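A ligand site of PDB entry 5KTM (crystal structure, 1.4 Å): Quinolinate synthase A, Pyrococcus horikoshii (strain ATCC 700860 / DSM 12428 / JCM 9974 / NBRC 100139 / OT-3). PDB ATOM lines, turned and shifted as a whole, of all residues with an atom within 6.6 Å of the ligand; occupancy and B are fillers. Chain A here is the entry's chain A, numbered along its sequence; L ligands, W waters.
SG of Cys 174 binds FE3 of the ligand, at 2.4 Å. N of Ala 88 sits close to S4 of the ligand (3.8 Å). The side-chain sulfur (SG) of Cys 87 is bound to an iron atom (FE1) of the ligand (2.4 Å). An iron atom (FE2) of the ligand is bound by the side-chain sulfur of Cys 260 (2.3 Å). S2 of the ligand sits close to ND2 of Asn 115, at 3.7 Å.
The backbone NH (N) of Cys 260 lies within hydrogen-bond range of the side-chain carboxylate (OE2) of Glu 235, at 2.8 Å. The side-chain sulfur of Cys 87 sits close to the backbone NH of Ala 90 (3.2 Å). The side-chain sulfur (SG) of Cys 174 lies close to a ring nitrogen (ND1) of His 177, 3.3 Å away. OE1 of Glu 202 sits at hydrogen-bond distance from ND1 of His 177 (3.0 Å). The side-chain hydroxyl (OH) of Tyr 113 sits at hydrogen-bond distance from the side-chain carboxylate (OE2) of Glu 202 (2.5 Å). The side-chain sulfur (SG) of Cys 174 sits close to the backbone NH (N) of Val 176 (3.4 Å). The backbone NH (N) of Gly 262 lies close to the side-chain sulfur (SG) of Cys 260. SG of Cys 87 lies close to N of Met 89, at 3.5 Å.
The side-chain carboxylate (OE1) of Glu 202 sits close to a sulfur (S2) of the ligand (3.7 Å). CE2 of Tyr 27 touches S1 of the ligand (3.8 Å). Val 62 touches the ligand (CG2 to S3, 3.9 Å). Met 89 touches the ligand (CE to S2, 3.7 Å). Tyr 175 touches the ligand. Val 176 touches the ligand (CG2 to S1, 3.999 Å). CE of Met 263 touches S3 of the ligand, at 3.9 Å. Within 4 Å of the ligand: Tyr 27, Val 62, Cys 87, Ala 88, Met 89, Asn 115, Cys 174, Tyr 175, Val 176, Glu 202, Cys 260 and Met 263. The nearest printed residue that does not touch the ligand is His 177 (4.5 Å).
Water W1 lies within hydrogen-bond range of O of Thr 86 (2.8 Å), N of Ala 88 (3.1 Å) and S4 of the ligand (3.4 Å).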
ATOM      1  N   HIS A  25      -9.546 -39.699  16.979  1.00  0.00           N
ATOM      2  CA  HIS A  25      -8.329 -38.938  16.760  1.00  0.00           C
ATOM      3  C   HIS A  25      -7.304 -39.252  17.844  1.00  0.00           C
ATOM      4  O   HIS A  25      -7.638 -39.663  18.964  1.00  0.00           O
ATOM      5  CB  HIS A  25      -8.631 -37.433  16.766  1.00  0.00           C
ATOM      6  CG  HIS A  25      -7.483 -36.602  16.310  1.00  0.00           C
ATOM      7  ND1 HIS A  25      -6.567 -36.046  17.187  1.00  0.00           N
ATOM      8  CD2 HIS A  25      -7.077 -36.248  15.064  1.00  0.00           C
ATOM      9  CE1 HIS A  25      -5.663 -35.372  16.498  1.00  0.00           C
ATOM     10  NE2 HIS A  25      -5.943 -35.493  15.210  1.00  0.00           N
ATOM     11  N   TYR A  27      -5.824 -37.373  19.714  1.00  0.00           N
ATOM     12  CA  TYR A  27      -5.936 -36.536  20.905  1.00  0.00           C
ATOM     13  C   TYR A  27      -7.128 -36.906  21.775  1.00  0.00           C
ATOM     14  O   TYR A  27      -7.420 -36.204  22.749  1.00  0.00           O
ATOM     15  CB  TYR A  27      -6.035 -35.047  20.535  1.00  0.00           C
ATOM     16  CG  TYR A  27      -4.880 -34.468  19.750  1.00  0.00           C
ATOM     17  CD1 TYR A  27      -3.639 -35.099  19.700  1.00  0.00           C
ATOM     18  CD2 TYR A  27      -5.033 -33.268  19.062  1.00  0.00           C
ATOM     19  CE1 TYR A  27      -2.595 -34.558  18.975  1.00  0.00           C
ATOM     20  CE2 TYR A  27      -3.994 -32.715  18.332  1.00  0.00           C
ATOM     21  CZ  TYR A  27      -2.766 -33.366  18.285  1.00  0.00           C
ATOM     22  OH  TYR A  27      -1.740 -32.810  17.558  1.00  0.00           O
ATOM     23  N   VAL A  62     -13.182 -33.719  16.449  1.00  0.00           N
ATOM     24  CA  VAL A  62     -13.862 -32.431  16.364  1.00  0.00           C
ATOM     25  C   VAL A  62     -14.673 -32.297  15.079  1.00  0.00           C
ATOM     26  O   VAL A  62     -14.535 -33.110  14.144  1.00  0.00           O
ATOM     27  CB  VAL A  62     -12.904 -31.240  16.555  1.00  0.00           C
ATOM     28  CG1 VAL A  62     -12.310 -31.264  17.962  1.00  0.00           C
ATOM     29  CG2 VAL A  62     -11.797 -31.284  15.521  1.00  0.00           C
ATOM     30  N   PHE A  64     -14.826 -30.511  12.259  1.00  0.00           N
ATOM     31  CA  PHE A  64     -14.316 -30.532  10.883  1.00  0.00           C
ATOM     32  C   PHE A  64     -13.860 -31.931  10.488  1.00  0.00           C
ATOM     33  O   PHE A  64     -13.909 -32.282   9.309  1.00  0.00           O
ATOM     34  CB  PHE A  64     -13.210 -29.493  10.669  1.00  0.00           C
ATOM     35  CG  PHE A  64     -11.852 -29.893  11.193  1.00  0.00           C
ATOM     36  CD1 PHE A  64     -11.040 -30.770  10.471  1.00  0.00           C
ATOM     37  CD2 PHE A  64     -11.350 -29.348  12.366  1.00  0.00           C
ATOM     38  CE1 PHE A  64      -9.790 -31.135  10.945  1.00  0.00           C
ATOM     39  CE2 PHE A  64     -10.092 -29.709  12.842  1.00  0.00           C
ATOM     40  CZ  PHE A  64      -9.310 -30.595  12.129  1.00  0.00           C
ATOM     41  N   MET A  65     -13.422 -32.731  11.458  1.00  0.00           N
ATOM     42  CA  MET A  65     -13.005 -34.097  11.172  1.00  0.00           C
ATOM     43  C   MET A  65     -14.191 -34.979  10.822  1.00  0.00           C
ATOM     44  O   MET A  65     -14.133 -35.785   9.888  1.00  0.00           O
ATOM     45  CB  MET A  65     -12.256 -34.665  12.371  1.00  0.00           C
ATOM     46  CG  MET A  65     -11.148 -33.763  12.840  1.00  0.00           C
ATOM     47  SD  MET A  65     -10.156 -34.531  14.128  1.00  0.00           S
ATOM     48  CE  MET A  65      -8.787 -33.360  14.165  1.00  0.00           C
ATOM     49  N   THR A  86     -15.217 -28.896  18.836  1.00  0.00           N
ATOM     50  CA  THR A  86     -14.912 -27.980  17.746  1.00  0.00           C
ATOM     51  C   THR A  86     -13.438 -27.597  17.795  1.00  0.00           C
ATOM     52  O   THR A  86     -12.762 -27.754  18.814  1.00  0.00           O
ATOM     53  CB  THR A  86     -15.780 -26.705  17.808  1.00  0.00           C
ATOM     54  OG1 THR A  86     -15.464 -25.968  19.006  1.00  0.00           O
ATOM     55  CG2 THR A  86     -17.267 -27.048  17.814  1.00  0.00           C
ATOM     56  N   CYS A  87     -12.943 -27.077  16.668  1.00  0.00           N
ATOM     57  CA  CYS A  87     -11.543 -26.695  16.511  1.00  0.00           C
ATOM     58  C   CYS A  87     -11.440 -25.178  16.481  1.00  0.00           C
ATOM     59  O   CYS A  87     -11.911 -24.535  15.538  1.00  0.00           O
ATOM     60  CB  CYS A  87     -10.968 -27.312  15.236  1.00  0.00           C
ATOM     61  SG  CYS A  87      -9.305 -26.717  14.844  1.00  0.00           S
ATOM     62  N   ALA A  88     -10.788 -24.607  17.495  1.00  0.00           N
ATOM     63  CA  ALA A  88     -10.644 -23.159  17.561  1.00  0.00           C
ATOM     64  C   ALA A  88      -9.839 -22.605  16.385  1.00  0.00           C
ATOM     65  O   ALA A  88     -10.091 -21.491  15.922  1.00  0.00           O
ATOM     66  CB  ALA A  88      -9.988 -22.751  18.874  1.00  0.00           C
ATOM     67  N   MET A  89      -8.870 -23.372  15.880  1.00  0.00           N
ATOM     68  CA  MET A  89      -8.074 -22.909  14.750  1.00  0.00           C
ATOM     69  C   MET A  89      -8.911 -22.870  13.476  1.00  0.00           C
ATOM     70  O   MET A  89      -8.932 -21.861  12.758  1.00  0.00           O
ATOM     71  CB  MET A  89      -6.841 -23.789  14.577  1.00  0.00           C
ATOM     72  CG  MET A  89      -5.887 -23.300  13.499  1.00  0.00           C
ATOM     73  SD  MET A  89      -5.907 -24.333  12.022  1.00  0.00           S
ATOM     74  CE  MET A  89      -5.009 -25.757  12.645  1.00  0.00           C
ATOM     75  N   ALA A  90      -9.627 -23.959  13.187  1.00  0.00           N
ATOM     76  CA  ALA A  90     -10.469 -24.004  11.996  1.00  0.00           C
ATOM     77  C   ALA A  90     -11.543 -22.919  12.007  1.00  0.00           C
ATOM     78  O   ALA A  90     -11.871 -22.351  10.967  1.00  0.00           O
ATOM     79  CB  ALA A  90     -11.109 -25.383  11.869  1.00  0.00           C
ATOM     80  N   TYR A 113      -5.185 -26.085   4.637  1.00  0.00           N
ATOM     81  CA  TYR A 113      -4.894 -27.164   5.572  1.00  0.00           C
ATOM     82  C   TYR A 113      -6.174 -27.947   5.842  1.00  0.00           C
ATOM     83  O   TYR A 113      -7.257 -27.364   5.942  1.00  0.00           O
ATOM     84  CB  TYR A 113      -4.435 -26.501   6.854  1.00  0.00           C
ATOM     85  CG  TYR A 113      -3.807 -27.357   7.922  1.00  0.00           C
ATOM     86  CD1 TYR A 113      -3.294 -28.623   7.654  1.00  0.00           C
ATOM     87  CD2 TYR A 113      -3.690 -26.864   9.198  1.00  0.00           C
ATOM     88  CE1 TYR A 113      -2.716 -29.379   8.676  1.00  0.00           C
ATOM     89  CE2 TYR A 113      -3.110 -27.571  10.200  1.00  0.00           C
ATOM     90  CZ  TYR A 113      -2.622 -28.833   9.948  1.00  0.00           C
ATOM     91  OH  TYR A 113      -2.045 -29.521  11.004  1.00  0.00           O
ATOM     92  N   ASN A 115      -7.125 -29.200   8.470  1.00  0.00           N
ATOM     93  CA  ASN A 115      -7.719 -28.674   9.690  1.00  0.00           C
ATOM     94  C   ASN A 115      -8.415 -27.364   9.371  1.00  0.00           C
ATOM     95  O   ASN A 115      -7.815 -26.287   9.486  1.00  0.00           O
ATOM     96  CB  ASN A 115      -6.659 -28.498  10.778  1.00  0.00           C
ATOM     97  CG  ASN A 115      -6.139 -29.816  11.314  1.00  0.00           C
ATOM     98  OD1 ASN A 115      -6.128 -30.831  10.628  1.00  0.00           O
ATOM     99  ND2 ASN A 115      -5.687 -29.801  12.565  1.00  0.00           N
ATOM    100  N   ASP A 150      -3.554 -21.998   9.396  1.00  0.00           N
ATOM    101  CA  ASP A 150      -2.506 -21.951  10.411  1.00  0.00           C
ATOM    102  C   ASP A 150      -1.268 -21.211   9.910  1.00  0.00           C
ATOM    103  O   ASP A 150      -0.575 -21.668   8.994  1.00  0.00           O
ATOM    104  CB  ASP A 150      -2.143 -23.362  10.860  1.00  0.00           C
ATOM    105  CG  ASP A 150      -1.301 -23.380  12.098  1.00  0.00           C
ATOM    106  OD1 ASP A 150      -1.853 -23.516  13.199  1.00  0.00           O
ATOM    107  OD2 ASP A 150      -0.078 -23.252  11.968  1.00  0.00           O
ATOM    108  N   HIS A 173      -4.104 -19.738  14.134  1.00  0.00           N
ATOM    109  CA  HIS A 173      -3.188 -20.572  14.903  1.00  0.00           C
ATOM    110  C   HIS A 173      -4.019 -21.506  15.769  1.00  0.00           C
ATOM    111  O   HIS A 173      -5.207 -21.286  15.979  1.00  0.00           O
ATOM    112  CB  HIS A 173      -2.309 -19.715  15.811  1.00  0.00           C
ATOM    113  CG  HIS A 173      -3.090 -18.999  16.876  1.00  0.00           C
ATOM    114  ND1 HIS A 173      -3.801 -17.847  16.625  1.00  0.00           N
ATOM    115  CD2 HIS A 173      -3.297 -19.298  18.184  1.00  0.00           C
ATOM    116  CE1 HIS A 173      -4.407 -17.464  17.731  1.00  0.00           C
ATOM    117  NE2 HIS A 173      -4.118 -18.319  18.689  1.00  0.00           N
ATOM    118  N   CYS A 174      -3.354 -22.549  16.280  1.00  0.00           N
ATOM    119  CA  CYS A 174      -3.904 -23.477  17.256  1.00  0.00           C
ATOM    120  C   CYS A 174      -3.394 -23.079  18.635  1.00  0.00           C
ATOM    121  O   CYS A 174      -2.182 -23.075  18.881  1.00  0.00           O
ATOM    122  CB  CYS A 174      -3.451 -24.887  16.922  1.00  0.00           C
ATOM    123  SG  CYS A 174      -3.702 -26.046  18.278  1.00  0.00           S
ATOM    124  N   TYR A 175      -4.321 -22.740  19.550  1.00  0.00           N
ATOM    125  CA  TYR A 175      -3.902 -22.294  20.873  1.00  0.00           C
ATOM    126  C   TYR A 175      -3.122 -23.364  21.628  1.00  0.00           C
ATOM    127  O   TYR A 175      -2.277 -23.035  22.467  1.00  0.00           O
ATOM    128  CB  TYR A 175      -5.100 -21.817  21.694  1.00  0.00           C
ATOM    129  CG  TYR A 175      -6.051 -22.903  22.183  1.00  0.00           C
ATOM    130  CD1 TYR A 175      -5.957 -23.408  23.481  1.00  0.00           C
ATOM    131  CD2 TYR A 175      -7.074 -23.383  21.365  1.00  0.00           C
ATOM    132  CE1 TYR A 175      -6.844 -24.383  23.940  1.00  0.00           C
ATOM    133  CE2 TYR A 175      -7.961 -24.359  21.824  1.00  0.00           C
ATOM    134  CZ  TYR A 175      -7.837 -24.855  23.112  1.00  0.00           C
ATOM    135  OH  TYR A 175      -8.713 -25.806  23.582  1.00  0.00           O
ATOM    136  N   VAL A 176      -3.383 -24.639  21.346  1.00  0.00           N
ATOM    137  CA  VAL A 176      -2.643 -25.697  22.022  1.00  0.00           C
ATOM    138  C   VAL A 176      -1.184 -25.657  21.610  1.00  0.00           C
ATOM    139  O   VAL A 176      -0.278 -25.590  22.458  1.00  0.00           O
ATOM    140  CB  VAL A 176      -3.276 -27.068  21.708  1.00  0.00           C
ATOM    141  CG1 VAL A 176      -2.492 -28.180  22.408  1.00  0.00           C
ATOM    142  CG2 VAL A 176      -4.744 -27.088  22.119  1.00  0.00           C
ATOM    143  N   HIS A 177      -0.927 -25.667  20.300  1.00  0.00           N
ATOM    144  CA  HIS A 177       0.463 -25.702  19.825  1.00  0.00           C
ATOM    145  C   HIS A 177       1.173 -24.375  20.019  1.00  0.00           C
ATOM    146  O   HIS A 177       2.399 -24.357  20.182  1.00  0.00           O
ATOM    147  CB  HIS A 177       0.508 -26.168  18.376  1.00  0.00           C
ATOM    148  CG  HIS A 177       0.162 -27.612  18.232  1.00  0.00           C
ATOM    149  ND1 HIS A 177      -1.089 -28.044  17.866  1.00  0.00           N
ATOM    150  CD2 HIS A 177       0.890 -28.727  18.477  1.00  0.00           C
ATOM    151  CE1 HIS A 177      -1.110 -29.363  17.862  1.00  0.00           C
ATOM    152  NE2 HIS A 177       0.074 -29.801  18.228  1.00  0.00           N
ATOM    153  N   GLU A 202       2.502 -26.978  13.762  1.00  0.00           N
ATOM    154  CA  GLU A 202       1.661 -25.910  14.291  1.00  0.00           C
ATOM    155  C   GLU A 202       2.329 -25.130  15.418  1.00  0.00           C
ATOM    156  O   GLU A 202       1.776 -24.121  15.865  1.00  0.00           O
ATOM    157  CB  GLU A 202       0.281 -26.433  14.723  1.00  0.00           C
ATOM    158  CG  GLU A 202      -0.595 -26.879  13.548  1.00  0.00           C
ATOM    159  CD  GLU A 202      -1.883 -27.567  14.001  1.00  0.00           C
ATOM    160  OE1 GLU A 202      -2.293 -27.371  15.173  1.00  0.00           O
ATOM    161  OE2 GLU A 202      -2.486 -28.307  13.202  1.00  0.00           O
ATOM    162  N   GLU A 235      -0.387 -32.008  21.497  1.00  0.00           N
ATOM    163  CA  GLU A 235      -1.427 -32.182  22.493  1.00  0.00           C
ATOM    164  C   GLU A 235      -1.136 -33.409  23.334  1.00  0.00           C
ATOM    165  O   GLU A 235      -0.707 -34.444  22.819  1.00  0.00           O
ATOM    166  CB  GLU A 235      -2.780 -32.319  21.791  1.00  0.00           C
ATOM    167  CG  GLU A 235      -3.981 -31.799  22.578  1.00  0.00           C
ATOM    168  CD  GLU A 235      -4.589 -32.810  23.518  1.00  0.00           C
ATOM    169  OE1 GLU A 235      -4.173 -34.000  23.522  1.00  0.00           O
ATOM    170  OE2 GLU A 235      -5.506 -32.424  24.264  1.00  0.00           O
ATOM    171  N   PHE A 259      -3.602 -28.935  26.118  1.00  0.00           N
ATOM    172  CA  PHE A 259      -4.883 -29.631  26.252  1.00  0.00           C
ATOM    173  C   PHE A 259      -5.877 -28.970  25.293  1.00  0.00           C
ATOM    174  O   PHE A 259      -6.091 -27.759  25.368  1.00  0.00           O
ATOM    175  CB  PHE A 259      -5.348 -29.487  27.718  1.00  0.00           C
ATOM    176  CG  PHE A 259      -6.715 -30.055  28.014  1.00  0.00           C
ATOM    177  CD1 PHE A 259      -6.849 -31.343  28.486  1.00  0.00           C
ATOM    178  CD2 PHE A 259      -7.852 -29.266  27.896  1.00  0.00           C
ATOM    179  CE1 PHE A 259      -8.095 -31.862  28.783  1.00  0.00           C
ATOM    180  CE2 PHE A 259      -9.098 -29.781  28.184  1.00  0.00           C
ATOM    181  CZ  PHE A 259      -9.216 -31.077  28.639  1.00  0.00           C
ATOM    182  N   CYS A 260      -6.467 -29.763  24.398  1.00  0.00           N
ATOM    183  CA  CYS A 260      -7.496 -29.259  23.488  1.00  0.00           C
ATOM    184  C   CYS A 260      -8.867 -29.479  24.103  1.00  0.00           C
ATOM    185  O   CYS A 260      -9.349 -30.616  24.160  1.00  0.00           O
ATOM    186  CB  CYS A 260      -7.436 -29.958  22.136  1.00  0.00           C
ATOM    187  SG  CYS A 260      -8.721 -29.342  21.015  1.00  0.00           S
ATOM    188  N   ILE A 261      -9.529 -28.381  24.494  1.00  0.00           N
ATOM    189  CA  ILE A 261     -10.849 -28.471  25.124  1.00  0.00           C
ATOM    190  C   ILE A 261     -11.850 -29.114  24.168  1.00  0.00           C
ATOM    191  O   ILE A 261     -12.679 -29.932  24.575  1.00  0.00           O
ATOM    192  CB  ILE A 261     -11.308 -27.088  25.613  1.00  0.00           C
ATOM    193  CG1 ILE A 261     -10.369 -26.565  26.707  1.00  0.00           C
ATOM    194  CG2 ILE A 261     -12.736 -27.109  26.154  1.00  0.00           C
ATOM    195  CD1 ILE A 261     -10.588 -25.101  27.089  1.00  0.00           C
ATOM    196  N   GLY A 262     -11.754 -28.789  22.872  1.00  0.00           N
ATOM    197  CA  GLY A 262     -12.693 -29.350  21.916  1.00  0.00           C
ATOM    198  C   GLY A 262     -12.602 -30.850  21.822  1.00  0.00           C
ATOM    199  O   GLY A 262     -13.621 -31.554  21.824  1.00  0.00           O
ATOM    200  N   MET A 263     -11.380 -31.382  21.756  1.00  0.00           N
ATOM    201  CA  MET A 263     -11.208 -32.831  21.712  1.00  0.00           C
ATOM    202  C   MET A 263     -11.811 -33.502  22.922  1.00  0.00           C
ATOM    203  O   MET A 263     -12.436 -34.575  22.823  1.00  0.00           O
ATOM    204  CB  MET A 263      -9.713 -33.160  21.641  1.00  0.00           C
ATOM    205  CG  MET A 263      -9.116 -32.932  20.279  1.00  0.00           C
ATOM    206  SD  MET A 263      -9.699 -34.163  19.099  1.00  0.00           S
ATOM    207  CE  MET A 263      -8.986 -33.519  17.607  1.00  0.00           C
HETATM  208 FE1  LIG L   1      -7.962 -27.598  16.567  1.00  0.00          FE
HETATM  209 FE2  LIG L   1      -7.711 -28.706  18.995  1.00  0.00          FE
HETATM  210 FE3  LIG L   1      -5.649 -27.303  17.865  1.00  0.00          FE
HETATM  211 FE4  LIG L   1      -6.425 -29.719  16.799  1.00  0.00          FE
HETATM  212  S1  LIG L   1      -5.527 -29.317  18.892  1.00  0.00           S
HETATM  213  S2  LIG L   1      -5.905 -27.765  15.676  1.00  0.00           S
HETATM  214  S3  LIG L   1      -8.683 -29.614  17.186  1.00  0.00           S
HETATM  215  S4  LIG L   1      -7.681 -26.476  18.487  1.00  0.00           S
HETATM  216  O   HOH W   1     -10.719 -26.387  20.068  1.00  0.00           O
